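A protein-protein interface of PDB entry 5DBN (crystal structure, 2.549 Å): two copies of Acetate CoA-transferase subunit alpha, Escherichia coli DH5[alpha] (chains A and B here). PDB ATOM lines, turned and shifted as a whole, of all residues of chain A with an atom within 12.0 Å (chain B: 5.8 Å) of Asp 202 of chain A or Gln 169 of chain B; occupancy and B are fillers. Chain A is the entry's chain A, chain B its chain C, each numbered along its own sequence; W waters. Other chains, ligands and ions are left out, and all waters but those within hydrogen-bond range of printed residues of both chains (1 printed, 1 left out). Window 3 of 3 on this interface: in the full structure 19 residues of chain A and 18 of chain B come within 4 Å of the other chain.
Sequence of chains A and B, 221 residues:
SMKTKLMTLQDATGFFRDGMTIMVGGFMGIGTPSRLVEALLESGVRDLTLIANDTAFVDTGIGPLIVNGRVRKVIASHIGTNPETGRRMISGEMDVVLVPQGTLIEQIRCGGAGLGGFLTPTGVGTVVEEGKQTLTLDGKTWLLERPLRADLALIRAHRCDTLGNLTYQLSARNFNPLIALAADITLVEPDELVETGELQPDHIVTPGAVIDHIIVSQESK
Of the 12 printed residues of chain B, 5 touch a printed residue of chain A.
Printed residues of chain B within 4 Å of His 203 of chain A: His 203 (3.5 Å). No residue of chain A comes within 4 Å of His 158 of chain B. Of the printed residues of chain A, Tyr 168 of chain B touches Asp 202 (3.4 Å). Gln 169 of chain B touches one residue of chain A. No residue of chain A comes within 4 Å of Ser 171 of chain B. No residue of chain A comes within 4 Å of Ala 172 of chain B. Arg 173 of chain B touches one residue of chain A. His 203 of chain B touches just one residue of chain A: His 203 (3.5 Å).
NE2 of His 158 of chain B sits at hydrogen-bond distance from OE1 of Gln 169 of chain B.
The side-chain carboxylate (OD1) of Asp 202 of chain A sits close to the backbone carbonyl oxygen (O) of Tyr 168 of chain B, 3.4 Å away. The backbone NH (N) of Leu 170 of chain B sits at hydrogen-bond distance from the side-chain carboxylate (OD2) of Asp 202 of chain A. The guanidinium group (NH2) of Arg 173 of chain B lies within salt-bridge range of the side-chain carboxylate (OD1) of Asp 202 of chain A (3.3 Å).
Among the printed residues, merely in contact across the chains: His 203 of chain A with His 203 of chain B (3.5 Å) and Asp 202 of chain A with Gln 169 of chain B (3.6 Å).
His 203 of chain A touches its own counterpart, His 203 of chain B. Positions printed for both chains: 167, 168, 173, 203 and 205.
Water W1 bridges O of His 203 of chain B (2.6 Å) and O of Asp 202 of chain A (2.8 Å).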
ATOM      1  N   ARG A 159      25.865  -6.594 -30.511  1.00  0.00           N
ATOM      2  CA  ARG A 159      27.314  -6.422 -30.534  1.00  0.00           C
ATOM      3  C   ARG A 159      28.016  -7.763 -30.329  1.00  0.00           C
ATOM      4  O   ARG A 159      27.473  -8.668 -29.698  1.00  0.00           O
ATOM      5  CB  ARG A 159      27.766  -5.432 -29.455  1.00  0.00           C
ATOM      6  CG  ARG A 159      27.500  -3.959 -29.758  1.00  0.00           C
ATOM      7  CD  ARG A 159      27.854  -3.090 -28.552  1.00  0.00           C
ATOM      8  NE  ARG A 159      27.847  -1.656 -28.848  1.00  0.00           N
ATOM      9  CZ  ARG A 159      26.827  -0.822 -28.656  1.00  0.00           C
ATOM     10  NH1 ARG A 159      25.674  -1.239 -28.152  1.00  0.00           N
ATOM     11  NH2 ARG A 159      26.973   0.459 -28.973  1.00  0.00           N
ATOM     12  N   ASP A 161      32.315  -9.295 -30.014  1.00  0.00           N
ATOM     13  CA  ASP A 161      33.758  -9.088 -30.107  1.00  0.00           C
ATOM     14  C   ASP A 161      34.410 -10.284 -30.797  1.00  0.00           C
ATOM     15  O   ASP A 161      33.730 -11.246 -31.147  1.00  0.00           O
ATOM     16  CB  ASP A 161      34.368  -8.847 -28.721  1.00  0.00           C
ATOM     17  CG  ASP A 161      34.229 -10.037 -27.794  1.00  0.00           C
ATOM     18  OD1 ASP A 161      33.555 -11.021 -28.166  1.00  0.00           O
ATOM     19  OD2 ASP A 161      34.794  -9.981 -26.680  1.00  0.00           O
ATOM     20  N   ASN A 165      31.916 -13.042 -27.564  1.00  0.00           N
ATOM     21  CA  ASN A 165      31.048 -12.548 -26.504  1.00  0.00           C
ATOM     22  C   ASN A 165      29.931 -11.730 -27.129  1.00  0.00           C
ATOM     23  O   ASN A 165      30.197 -10.834 -27.927  1.00  0.00           O
ATOM     24  CB  ASN A 165      31.828 -11.698 -25.496  1.00  0.00           C
ATOM     25  CG  ASN A 165      32.834 -12.507 -24.702  1.00  0.00           C
ATOM     26  OD1 ASN A 165      32.514 -13.568 -24.164  1.00  0.00           O
ATOM     27  ND2 ASN A 165      34.059 -12.002 -24.614  1.00  0.00           N
ATOM     28  N   LEU A 166      28.686 -12.040 -26.775  1.00  0.00           N
ATOM     29  CA  LEU A 166      27.530 -11.410 -27.413  1.00  0.00           C
ATOM     30  C   LEU A 166      26.690 -10.571 -26.458  1.00  0.00           C
ATOM     31  O   LEU A 166      26.553 -10.895 -25.277  1.00  0.00           O
ATOM     32  CB  LEU A 166      26.628 -12.470 -28.047  1.00  0.00           C
ATOM     33  CG  LEU A 166      27.294 -13.477 -28.985  1.00  0.00           C
ATOM     34  CD1 LEU A 166      26.252 -14.468 -29.488  1.00  0.00           C
ATOM     35  CD2 LEU A 166      27.994 -12.775 -30.144  1.00  0.00           C
ATOM     36  N   THR A 167      26.129  -9.492 -26.996  1.00  0.00           N
ATOM     37  CA  THR A 167      25.049  -8.759 -26.347  1.00  0.00           C
ATOM     38  C   THR A 167      23.864  -8.717 -27.310  1.00  0.00           C
ATOM     39  O   THR A 167      24.034  -8.921 -28.514  1.00  0.00           O
ATOM     40  CB  THR A 167      25.460  -7.331 -25.970  1.00  0.00           C
ATOM     41  OG1 THR A 167      25.644  -6.556 -27.160  1.00  0.00           O
ATOM     42  CG2 THR A 167      26.747  -7.337 -25.150  1.00  0.00           C
ATOM     43  N   TYR A 168      22.672  -8.453 -26.781  1.00  0.00           N
ATOM     44  CA  TYR A 168      21.460  -8.399 -27.596  1.00  0.00           C
ATOM     45  C   TYR A 168      20.717  -7.091 -27.364  1.00  0.00           C
ATOM     46  O   TYR A 168      20.957  -6.403 -26.372  1.00  0.00           O
ATOM     47  CB  TYR A 168      20.552  -9.588 -27.283  1.00  0.00           C
ATOM     48  CG  TYR A 168      21.236 -10.928 -27.421  1.00  0.00           C
ATOM     49  CD1 TYR A 168      21.922 -11.488 -26.354  1.00  0.00           C
ATOM     50  CD2 TYR A 168      21.198 -11.632 -28.617  1.00  0.00           C
ATOM     51  CE1 TYR A 168      22.548 -12.711 -26.469  1.00  0.00           C
ATOM     52  CE2 TYR A 168      21.822 -12.858 -28.742  1.00  0.00           C
ATOM     53  CZ  TYR A 168      22.495 -13.392 -27.662  1.00  0.00           C
ATOM     54  OH  TYR A 168      23.123 -14.610 -27.767  1.00  0.00           O
ATOM     55  N   ARG A 173      16.329 -10.575 -28.453  1.00  0.00           N
ATOM     56  CA  ARG A 173      17.058 -11.605 -27.719  1.00  0.00           C
ATOM     57  C   ARG A 173      16.354 -12.960 -27.801  1.00  0.00           C
ATOM     58  O   ARG A 173      16.849 -13.881 -28.448  1.00  0.00           O
ATOM     59  CB  ARG A 173      17.235 -11.183 -26.257  1.00  0.00           C
ATOM     60  CG  ARG A 173      18.162 -12.085 -25.456  1.00  0.00           C
ATOM     61  CD  ARG A 173      18.244 -11.659 -23.997  1.00  0.00           C
ATOM     62  NE  ARG A 173      18.697 -10.278 -23.846  1.00  0.00           N
ATOM     63  CZ  ARG A 173      19.090  -9.738 -22.696  1.00  0.00           C
ATOM     64  NH1 ARG A 173      19.099 -10.461 -21.583  1.00  0.00           N
ATOM     65  NH2 ARG A 173      19.482  -8.473 -22.657  1.00  0.00           N
ATOM     66  N   THR A 196      37.729  -6.905 -28.415  1.00  0.00           N
ATOM     67  CA  THR A 196      37.688  -7.587 -27.133  1.00  0.00           C
ATOM     68  C   THR A 196      38.059  -6.582 -26.051  1.00  0.00           C
ATOM     69  O   THR A 196      39.135  -5.982 -26.094  1.00  0.00           O
ATOM     70  CB  THR A 196      38.642  -8.795 -27.091  1.00  0.00           C
ATOM     71  OG1 THR A 196      38.294  -9.714 -28.134  1.00  0.00           O
ATOM     72  CG2 THR A 196      38.554  -9.507 -25.751  1.00  0.00           C
ATOM     73  N   GLY A 197      37.155  -6.396 -25.094  1.00  0.00           N
ATOM     74  CA  GLY A 197      37.342  -5.422 -24.035  1.00  0.00           C
ATOM     75  C   GLY A 197      36.305  -4.320 -24.130  1.00  0.00           C
ATOM     76  O   GLY A 197      36.037  -3.624 -23.153  1.00  0.00           O
ATOM     77  N   GLU A 198      35.720  -4.161 -25.316  1.00  0.00           N
ATOM     78  CA  GLU A 198      34.709  -3.133 -25.537  1.00  0.00           C
ATOM     79  C   GLU A 198      33.381  -3.536 -24.902  1.00  0.00           C
ATOM     80  O   GLU A 198      32.563  -2.680 -24.564  1.00  0.00           O
ATOM     81  CB  GLU A 198      34.522  -2.880 -27.036  1.00  0.00           C
ATOM     82  N   LEU A 199      33.174  -4.839 -24.742  1.00  0.00           N
ATOM     83  CA  LEU A 199      32.005  -5.348 -24.033  1.00  0.00           C
ATOM     84  C   LEU A 199      32.409  -5.659 -22.600  1.00  0.00           C
ATOM     85  O   LEU A 199      33.238  -6.538 -22.358  1.00  0.00           O
ATOM     86  CB  LEU A 199      31.439  -6.595 -24.717  1.00  0.00           C
ATOM     87  CG  LEU A 199      31.076  -6.452 -26.199  1.00  0.00           C
ATOM     88  CD1 LEU A 199      30.477  -7.747 -26.731  1.00  0.00           C
ATOM     89  CD2 LEU A 199      30.125  -5.287 -26.432  1.00  0.00           C
ATOM     90  N   GLN A 200      31.823  -4.937 -21.650  1.00  0.00           N
ATOM     91  CA  GLN A 200      32.151  -5.123 -20.243  1.00  0.00           C
ATOM     92  C   GLN A 200      31.723  -6.514 -19.775  1.00  0.00           C
ATOM     93  O   GLN A 200      30.713  -7.039 -20.244  1.00  0.00           O
ATOM     94  CB  GLN A 200      31.486  -4.045 -19.387  1.00  0.00           C
ATOM     95  CG  GLN A 200      32.059  -2.652 -19.599  1.00  0.00           C
ATOM     96  CD  GLN A 200      33.513  -2.554 -19.183  1.00  0.00           C
ATOM     97  OE1 GLN A 200      34.392  -2.316 -20.013  1.00  0.00           O
ATOM     98  NE2 GLN A 200      33.775  -2.743 -17.894  1.00  0.00           N
ATOM     99  N   PRO A 201      32.496  -7.117 -18.854  1.00  0.00           N
ATOM    100  CA  PRO A 201      32.182  -8.459 -18.348  1.00  0.00           C
ATOM    101  C   PRO A 201      30.759  -8.610 -17.807  1.00  0.00           C
ATOM    102  O   PRO A 201      30.183  -9.693 -17.929  1.00  0.00           O
ATOM    103  CB  PRO A 201      33.205  -8.654 -17.225  1.00  0.00           C
ATOM    104  CG  PRO A 201      34.353  -7.810 -17.614  1.00  0.00           C
ATOM    105  CD  PRO A 201      33.769  -6.613 -18.302  1.00  0.00           C
ATOM    106  N   ASP A 202      30.206  -7.547 -17.228  1.00  0.00           N
ATOM    107  CA  ASP A 202      28.874  -7.602 -16.628  1.00  0.00           C
ATOM    108  C   ASP A 202      27.770  -7.245 -17.622  1.00  0.00           C
ATOM    109  O   ASP A 202      26.606  -7.125 -17.243  1.00  0.00           O
ATOM    110  CB  ASP A 202      28.796  -6.657 -15.424  1.00  0.00           C
ATOM    111  CG  ASP A 202      29.418  -7.248 -14.173  1.00  0.00           C
ATOM    112  OD1 ASP A 202      29.101  -8.410 -13.844  1.00  0.00           O
ATOM    113  OD2 ASP A 202      30.222  -6.548 -13.519  1.00  0.00           O
ATOM    114  N   HIS A 203      28.134  -7.088 -18.891  1.00  0.00           N
ATOM    115  CA  HIS A 203      27.162  -6.764 -19.935  1.00  0.00           C
ATOM    116  C   HIS A 203      26.990  -7.899 -20.938  1.00  0.00           C
ATOM    117  O   HIS A 203      26.011  -7.939 -21.682  1.00  0.00           O
ATOM    118  CB  HIS A 203      27.588  -5.490 -20.665  1.00  0.00           C
ATOM    119  CG  HIS A 203      27.477  -4.254 -19.831  1.00  0.00           C
ATOM    120  ND1 HIS A 203      28.131  -3.083 -20.145  1.00  0.00           N
ATOM    121  CD2 HIS A 203      26.786  -4.005 -18.692  1.00  0.00           C
ATOM    122  CE1 HIS A 203      27.849  -2.167 -19.236  1.00  0.00           C
ATOM    123  NE2 HIS A 203      27.036  -2.701 -18.344  1.00  0.00           N
ATOM    124  N   ILE A 204      27.942  -8.824 -20.951  1.00  0.00           N
ATOM    125  CA  ILE A 204      27.916  -9.937 -21.890  1.00  0.00           C
ATOM    126  C   ILE A 204      26.844 -10.941 -21.489  1.00  0.00           C
ATOM    127  O   ILE A 204      26.799 -11.390 -20.345  1.00  0.00           O
ATOM    128  CB  ILE A 204      29.291 -10.631 -21.964  1.00  0.00           C
ATOM    129  CG1 ILE A 204      30.336  -9.662 -22.520  1.00  0.00           C
ATOM    130  CG2 ILE A 204      29.226 -11.899 -22.820  1.00  0.00           C
ATOM    131  CD1 ILE A 204      31.762 -10.075 -22.242  1.00  0.00           C
ATOM    132  N   VAL A 205      25.996 -11.295 -22.450  1.00  0.00           N
ATOM    133  CA  VAL A 205      24.890 -12.217 -22.215  1.00  0.00           C
ATOM    134  C   VAL A 205      25.283 -13.649 -22.574  1.00  0.00           C
ATOM    135  O   VAL A 205      25.029 -14.580 -21.811  1.00  0.00           O
ATOM    136  CB  VAL A 205      23.645 -11.813 -23.037  1.00  0.00           C
ATOM    137  CG1 VAL A 205      22.486 -12.761 -22.765  1.00  0.00           C
ATOM    138  CG2 VAL A 205      23.242 -10.377 -22.728  1.00  0.00           C
ATOM    139  N   THR A 206      25.898 -13.811 -23.741  1.00  0.00           N
ATOM    140  CA  THR A 206      26.360 -15.114 -24.206  1.00  0.00           C
ATOM    141  C   THR A 206      27.882 -15.119 -24.306  1.00  0.00           C
ATOM    142  O   THR A 206      28.446 -14.422 -25.149  1.00  0.00           O
ATOM    143  CB  THR A 206      25.751 -15.469 -25.578  1.00  0.00           C
ATOM    144  OG1 THR A 206      24.320 -15.433 -25.492  1.00  0.00           O
ATOM    145  CG2 THR A 206      26.204 -16.852 -26.038  1.00  0.00           C
ATOM    146  N   PRO A 207      28.561 -15.897 -23.444  1.00  0.00           N
ATOM    147  CA  PRO A 207      30.026 -15.925 -23.517  1.00  0.00           C
ATOM    148  C   PRO A 207      30.536 -16.573 -24.804  1.00  0.00           C
ATOM    149  O   PRO A 207      29.872 -17.446 -25.363  1.00  0.00           O
ATOM    150  CB  PRO A 207      30.426 -16.746 -22.290  1.00  0.00           C
ATOM    151  CG  PRO A 207      29.238 -17.586 -21.987  1.00  0.00           C
ATOM    152  CD  PRO A 207      28.045 -16.773 -22.376  1.00  0.00           C
ATOM    153  N   GLY A 208      31.710 -16.141 -25.259  1.00  0.00           N
ATOM    154  CA  GLY A 208      32.252 -16.579 -26.535  1.00  0.00           C
ATOM    155  C   GLY A 208      32.590 -18.058 -26.600  1.00  0.00           C
ATOM    156  O   GLY A 208      32.774 -18.609 -27.685  1.00  0.00           O
ATOM    157  N   ARG B 156      22.106  -9.487  -2.399  1.00  0.00           N
ATOM    158  CA  ARG B 156      22.974  -8.331  -2.594  1.00  0.00           C
ATOM    159  C   ARG B 156      23.052  -7.996  -4.074  1.00  0.00           C
ATOM    160  O   ARG B 156      23.169  -8.888  -4.916  1.00  0.00           O
ATOM    161  CB  ARG B 156      24.377  -8.588  -2.041  1.00  0.00           C
ATOM    162  CG  ARG B 156      25.293  -7.371  -2.103  1.00  0.00           C
ATOM    163  CD  ARG B 156      26.758  -7.754  -2.003  1.00  0.00           C
ATOM    164  NE  ARG B 156      27.637  -6.677  -2.451  1.00  0.00           N
ATOM    165  CZ  ARG B 156      28.941  -6.816  -2.680  1.00  0.00           C
ATOM    166  NH1 ARG B 156      29.532  -7.991  -2.499  1.00  0.00           N
ATOM    167  NH2 ARG B 156      29.657  -5.778  -3.090  1.00  0.00           N
ATOM    168  N   HIS B 158      24.595  -4.754  -6.978  1.00  0.00           N
ATOM    169  CA  HIS B 158      25.508  -3.637  -7.152  1.00  0.00           C
ATOM    170  C   HIS B 158      24.688  -2.355  -7.265  1.00  0.00           C
ATOM    171  O   HIS B 158      24.713  -1.509  -6.370  1.00  0.00           O
ATOM    172  CB  HIS B 158      26.387  -3.840  -8.385  1.00  0.00           C
ATOM    173  CG  HIS B 158      27.449  -2.799  -8.543  1.00  0.00           C
ATOM    174  ND1 HIS B 158      27.629  -2.085  -9.709  1.00  0.00           N
ATOM    175  CD2 HIS B 158      28.392  -2.352  -7.680  1.00  0.00           C
ATOM    176  CE1 HIS B 158      28.638  -1.244  -9.558  1.00  0.00           C
ATOM    177  NE2 HIS B 158      29.117  -1.387  -8.334  1.00  0.00           N
ATOM    178  N   THR B 167      21.358  -4.916 -11.035  1.00  0.00           N
ATOM    179  CA  THR B 167      22.559  -5.360 -11.730  1.00  0.00           C
ATOM    180  C   THR B 167      23.513  -5.880 -10.668  1.00  0.00           C
ATOM    181  O   THR B 167      23.370  -5.545  -9.491  1.00  0.00           O
ATOM    182  CB  THR B 167      23.242  -4.241 -12.531  1.00  0.00           C
ATOM    183  OG1 THR B 167      23.797  -3.279 -11.628  1.00  0.00           O
ATOM    184  CG2 THR B 167      22.259  -3.564 -13.471  1.00  0.00           C
ATOM    185  N   TYR B 168      24.485  -6.687 -11.084  1.00  0.00           N
ATOM    186  CA  TYR B 168      25.461  -7.263 -10.165  1.00  0.00           C
ATOM    187  C   TYR B 168      26.881  -6.982 -10.639  1.00  0.00           C
ATOM    188  O   TYR B 168      27.095  -6.619 -11.795  1.00  0.00           O
ATOM    189  CB  TYR B 168      25.241  -8.769 -10.023  1.00  0.00           C
ATOM    190  CG  TYR B 168      23.842  -9.146  -9.594  1.00  0.00           C
ATOM    191  CD1 TYR B 168      23.511  -9.241  -8.249  1.00  0.00           C
ATOM    192  CD2 TYR B 168      22.854  -9.414 -10.530  1.00  0.00           C
ATOM    193  CE1 TYR B 168      22.238  -9.590  -7.849  1.00  0.00           C
ATOM    194  CE2 TYR B 168      21.574  -9.765 -10.139  1.00  0.00           C
ATOM    195  CZ  TYR B 168      21.274  -9.851  -8.795  1.00  0.00           C
ATOM    196  OH  TYR B 168      20.004 -10.198  -8.392  1.00  0.00           O
ATOM    197  N   GLN B 169      27.843  -7.146  -9.734  1.00  0.00           N
ATOM    198  CA  GLN B 169      29.236  -6.829 -10.026  1.00  0.00           C
ATOM    199  C   GLN B 169      30.145  -8.050  -9.920  1.00  0.00           C
ATOM    200  O   GLN B 169      30.289  -8.643  -8.849  1.00  0.00           O
ATOM    201  CB  GLN B 169      29.736  -5.739  -9.079  1.00  0.00           C
ATOM    202  CG  GLN B 169      31.138  -5.254  -9.400  1.00  0.00           C
ATOM    203  CD  GLN B 169      31.473  -3.949  -8.708  1.00  0.00           C
ATOM    204  OE1 GLN B 169      31.655  -2.919  -9.356  1.00  0.00           O
ATOM    205  NE2 GLN B 169      31.574  -3.989  -7.386  1.00  0.00           N
ATOM    206  N   LEU B 170      30.755  -8.412 -11.047  1.00  0.00           N
ATOM    207  CA  LEU B 170      31.756  -9.471 -11.104  1.00  0.00           C
ATOM    208  C   LEU B 170      31.234 -10.789 -10.512  1.00  0.00           C
ATOM    209  O   LEU B 170      30.128 -11.218 -10.840  1.00  0.00           O
ATOM    210  CB  LEU B 170      33.029  -9.004 -10.393  1.00  0.00           C
ATOM    211  CG  LEU B 170      33.614  -7.696 -10.945  1.00  0.00           C
ATOM    212  CD1 LEU B 170      34.785  -7.222 -10.102  1.00  0.00           C
ATOM    213  CD2 LEU B 170      34.041  -7.848 -12.401  1.00  0.00           C
ATOM    214  N   SER B 171      32.018 -11.428  -9.645  1.00  0.00           N
ATOM    215  CA  SER B 171      31.676 -12.761  -9.155  1.00  0.00           C
ATOM    216  C   SER B 171      30.769 -12.721  -7.925  1.00  0.00           C
ATOM    217  O   SER B 171      30.582 -13.736  -7.254  1.00  0.00           O
ATOM    218  CB  SER B 171      32.950 -13.547  -8.832  1.00  0.00           C
ATOM    219  OG  SER B 171      33.626 -13.000  -7.714  1.00  0.00           O
ATOM    220  N   ALA B 172      30.204 -11.551  -7.639  1.00  0.00           N
ATOM    221  CA  ALA B 172      29.261 -11.402  -6.534  1.00  0.00           C
ATOM    222  C   ALA B 172      27.842 -11.762  -6.974  1.00  0.00           C
ATOM    223  O   ALA B 172      26.902 -11.690  -6.181  1.00  0.00           O
ATOM    224  CB  ALA B 172      29.301  -9.988  -5.991  1.00  0.00           C
ATOM    225  N   ARG B 173      27.688 -12.132  -8.244  1.00  0.00           N
ATOM    226  CA  ARG B 173      26.379 -12.489  -8.787  1.00  0.00           C
ATOM    227  C   ARG B 173      25.935 -13.875  -8.309  1.00  0.00           C
ATOM    228  O   ARG B 173      24.999 -13.991  -7.519  1.00  0.00           O
ATOM    229  CB  ARG B 173      26.409 -12.441 -10.318  1.00  0.00           C
ATOM    230  CG  ARG B 173      25.044 -12.598 -10.965  1.00  0.00           C
ATOM    231  CD  ARG B 173      25.123 -12.621 -12.484  1.00  0.00           C
ATOM    232  NE  ARG B 173      25.745 -11.418 -13.027  1.00  0.00           N
ATOM    233  CZ  ARG B 173      25.712 -11.071 -14.311  1.00  0.00           C
ATOM    234  NH1 ARG B 173      25.077 -11.832 -15.193  1.00  0.00           N
ATOM    235  NH2 ARG B 173      26.307  -9.956 -14.714  1.00  0.00           N
ATOM    236  N   ASP B 191      24.374  -1.932  -3.299  1.00  0.00           N
ATOM    237  CA  ASP B 191      25.533  -1.099  -2.995  1.00  0.00           C
ATOM    238  C   ASP B 191      25.231   0.347  -3.358  1.00  0.00           C
ATOM    239  O   ASP B 191      25.734   1.277  -2.726  1.00  0.00           O
ATOM    240  CB  ASP B 191      26.773  -1.574  -3.762  1.00  0.00           C
ATOM    241  CG  ASP B 191      27.095  -3.035  -3.517  1.00  0.00           C
ATOM    242  OD1 ASP B 191      26.682  -3.572  -2.467  1.00  0.00           O
ATOM    243  OD2 ASP B 191      27.763  -3.647  -4.379  1.00  0.00           O
ATOM    244  N   HIS B 203      20.807  -4.118 -19.610  1.00  0.00           N
ATOM    245  CA  HIS B 203      21.841  -4.274 -18.586  1.00  0.00           C
ATOM    246  C   HIS B 203      21.272  -4.865 -17.296  1.00  0.00           C
ATOM    247  O   HIS B 203      22.019  -5.329 -16.439  1.00  0.00           O
ATOM    248  CB  HIS B 203      22.513  -2.933 -18.287  1.00  0.00           C
ATOM    249  CG  HIS B 203      23.391  -2.433 -19.392  1.00  0.00           C
ATOM    250  ND1 HIS B 203      23.794  -1.119 -19.485  1.00  0.00           N
ATOM    251  CD2 HIS B 203      23.951  -3.074 -20.445  1.00  0.00           C
ATOM    252  CE1 HIS B 203      24.559  -0.969 -20.552  1.00  0.00           C
ATOM    253  NE2 HIS B 203      24.670  -2.141 -21.152  1.00  0.00           N
ATOM    254  N   VAL B 205      19.768  -7.440 -14.829  1.00  0.00           N
ATOM    255  CA  VAL B 205      19.889  -8.889 -14.691  1.00  0.00           C
ATOM    256  C   VAL B 205      18.653  -9.481 -14.025  1.00  0.00           C
ATOM    257  O   VAL B 205      18.128 -10.498 -14.475  1.00  0.00           O
ATOM    258  CB  VAL B 205      21.139  -9.268 -13.872  1.00  0.00           C
ATOM    259  CG1 VAL B 205      21.278 -10.780 -13.766  1.00  0.00           C
ATOM    260  CG2 VAL B 205      22.385  -8.667 -14.500  1.00  0.00           C
HETATM  261  O   HOH W   1      24.491  -5.947 -15.929  1.00  0.00           O
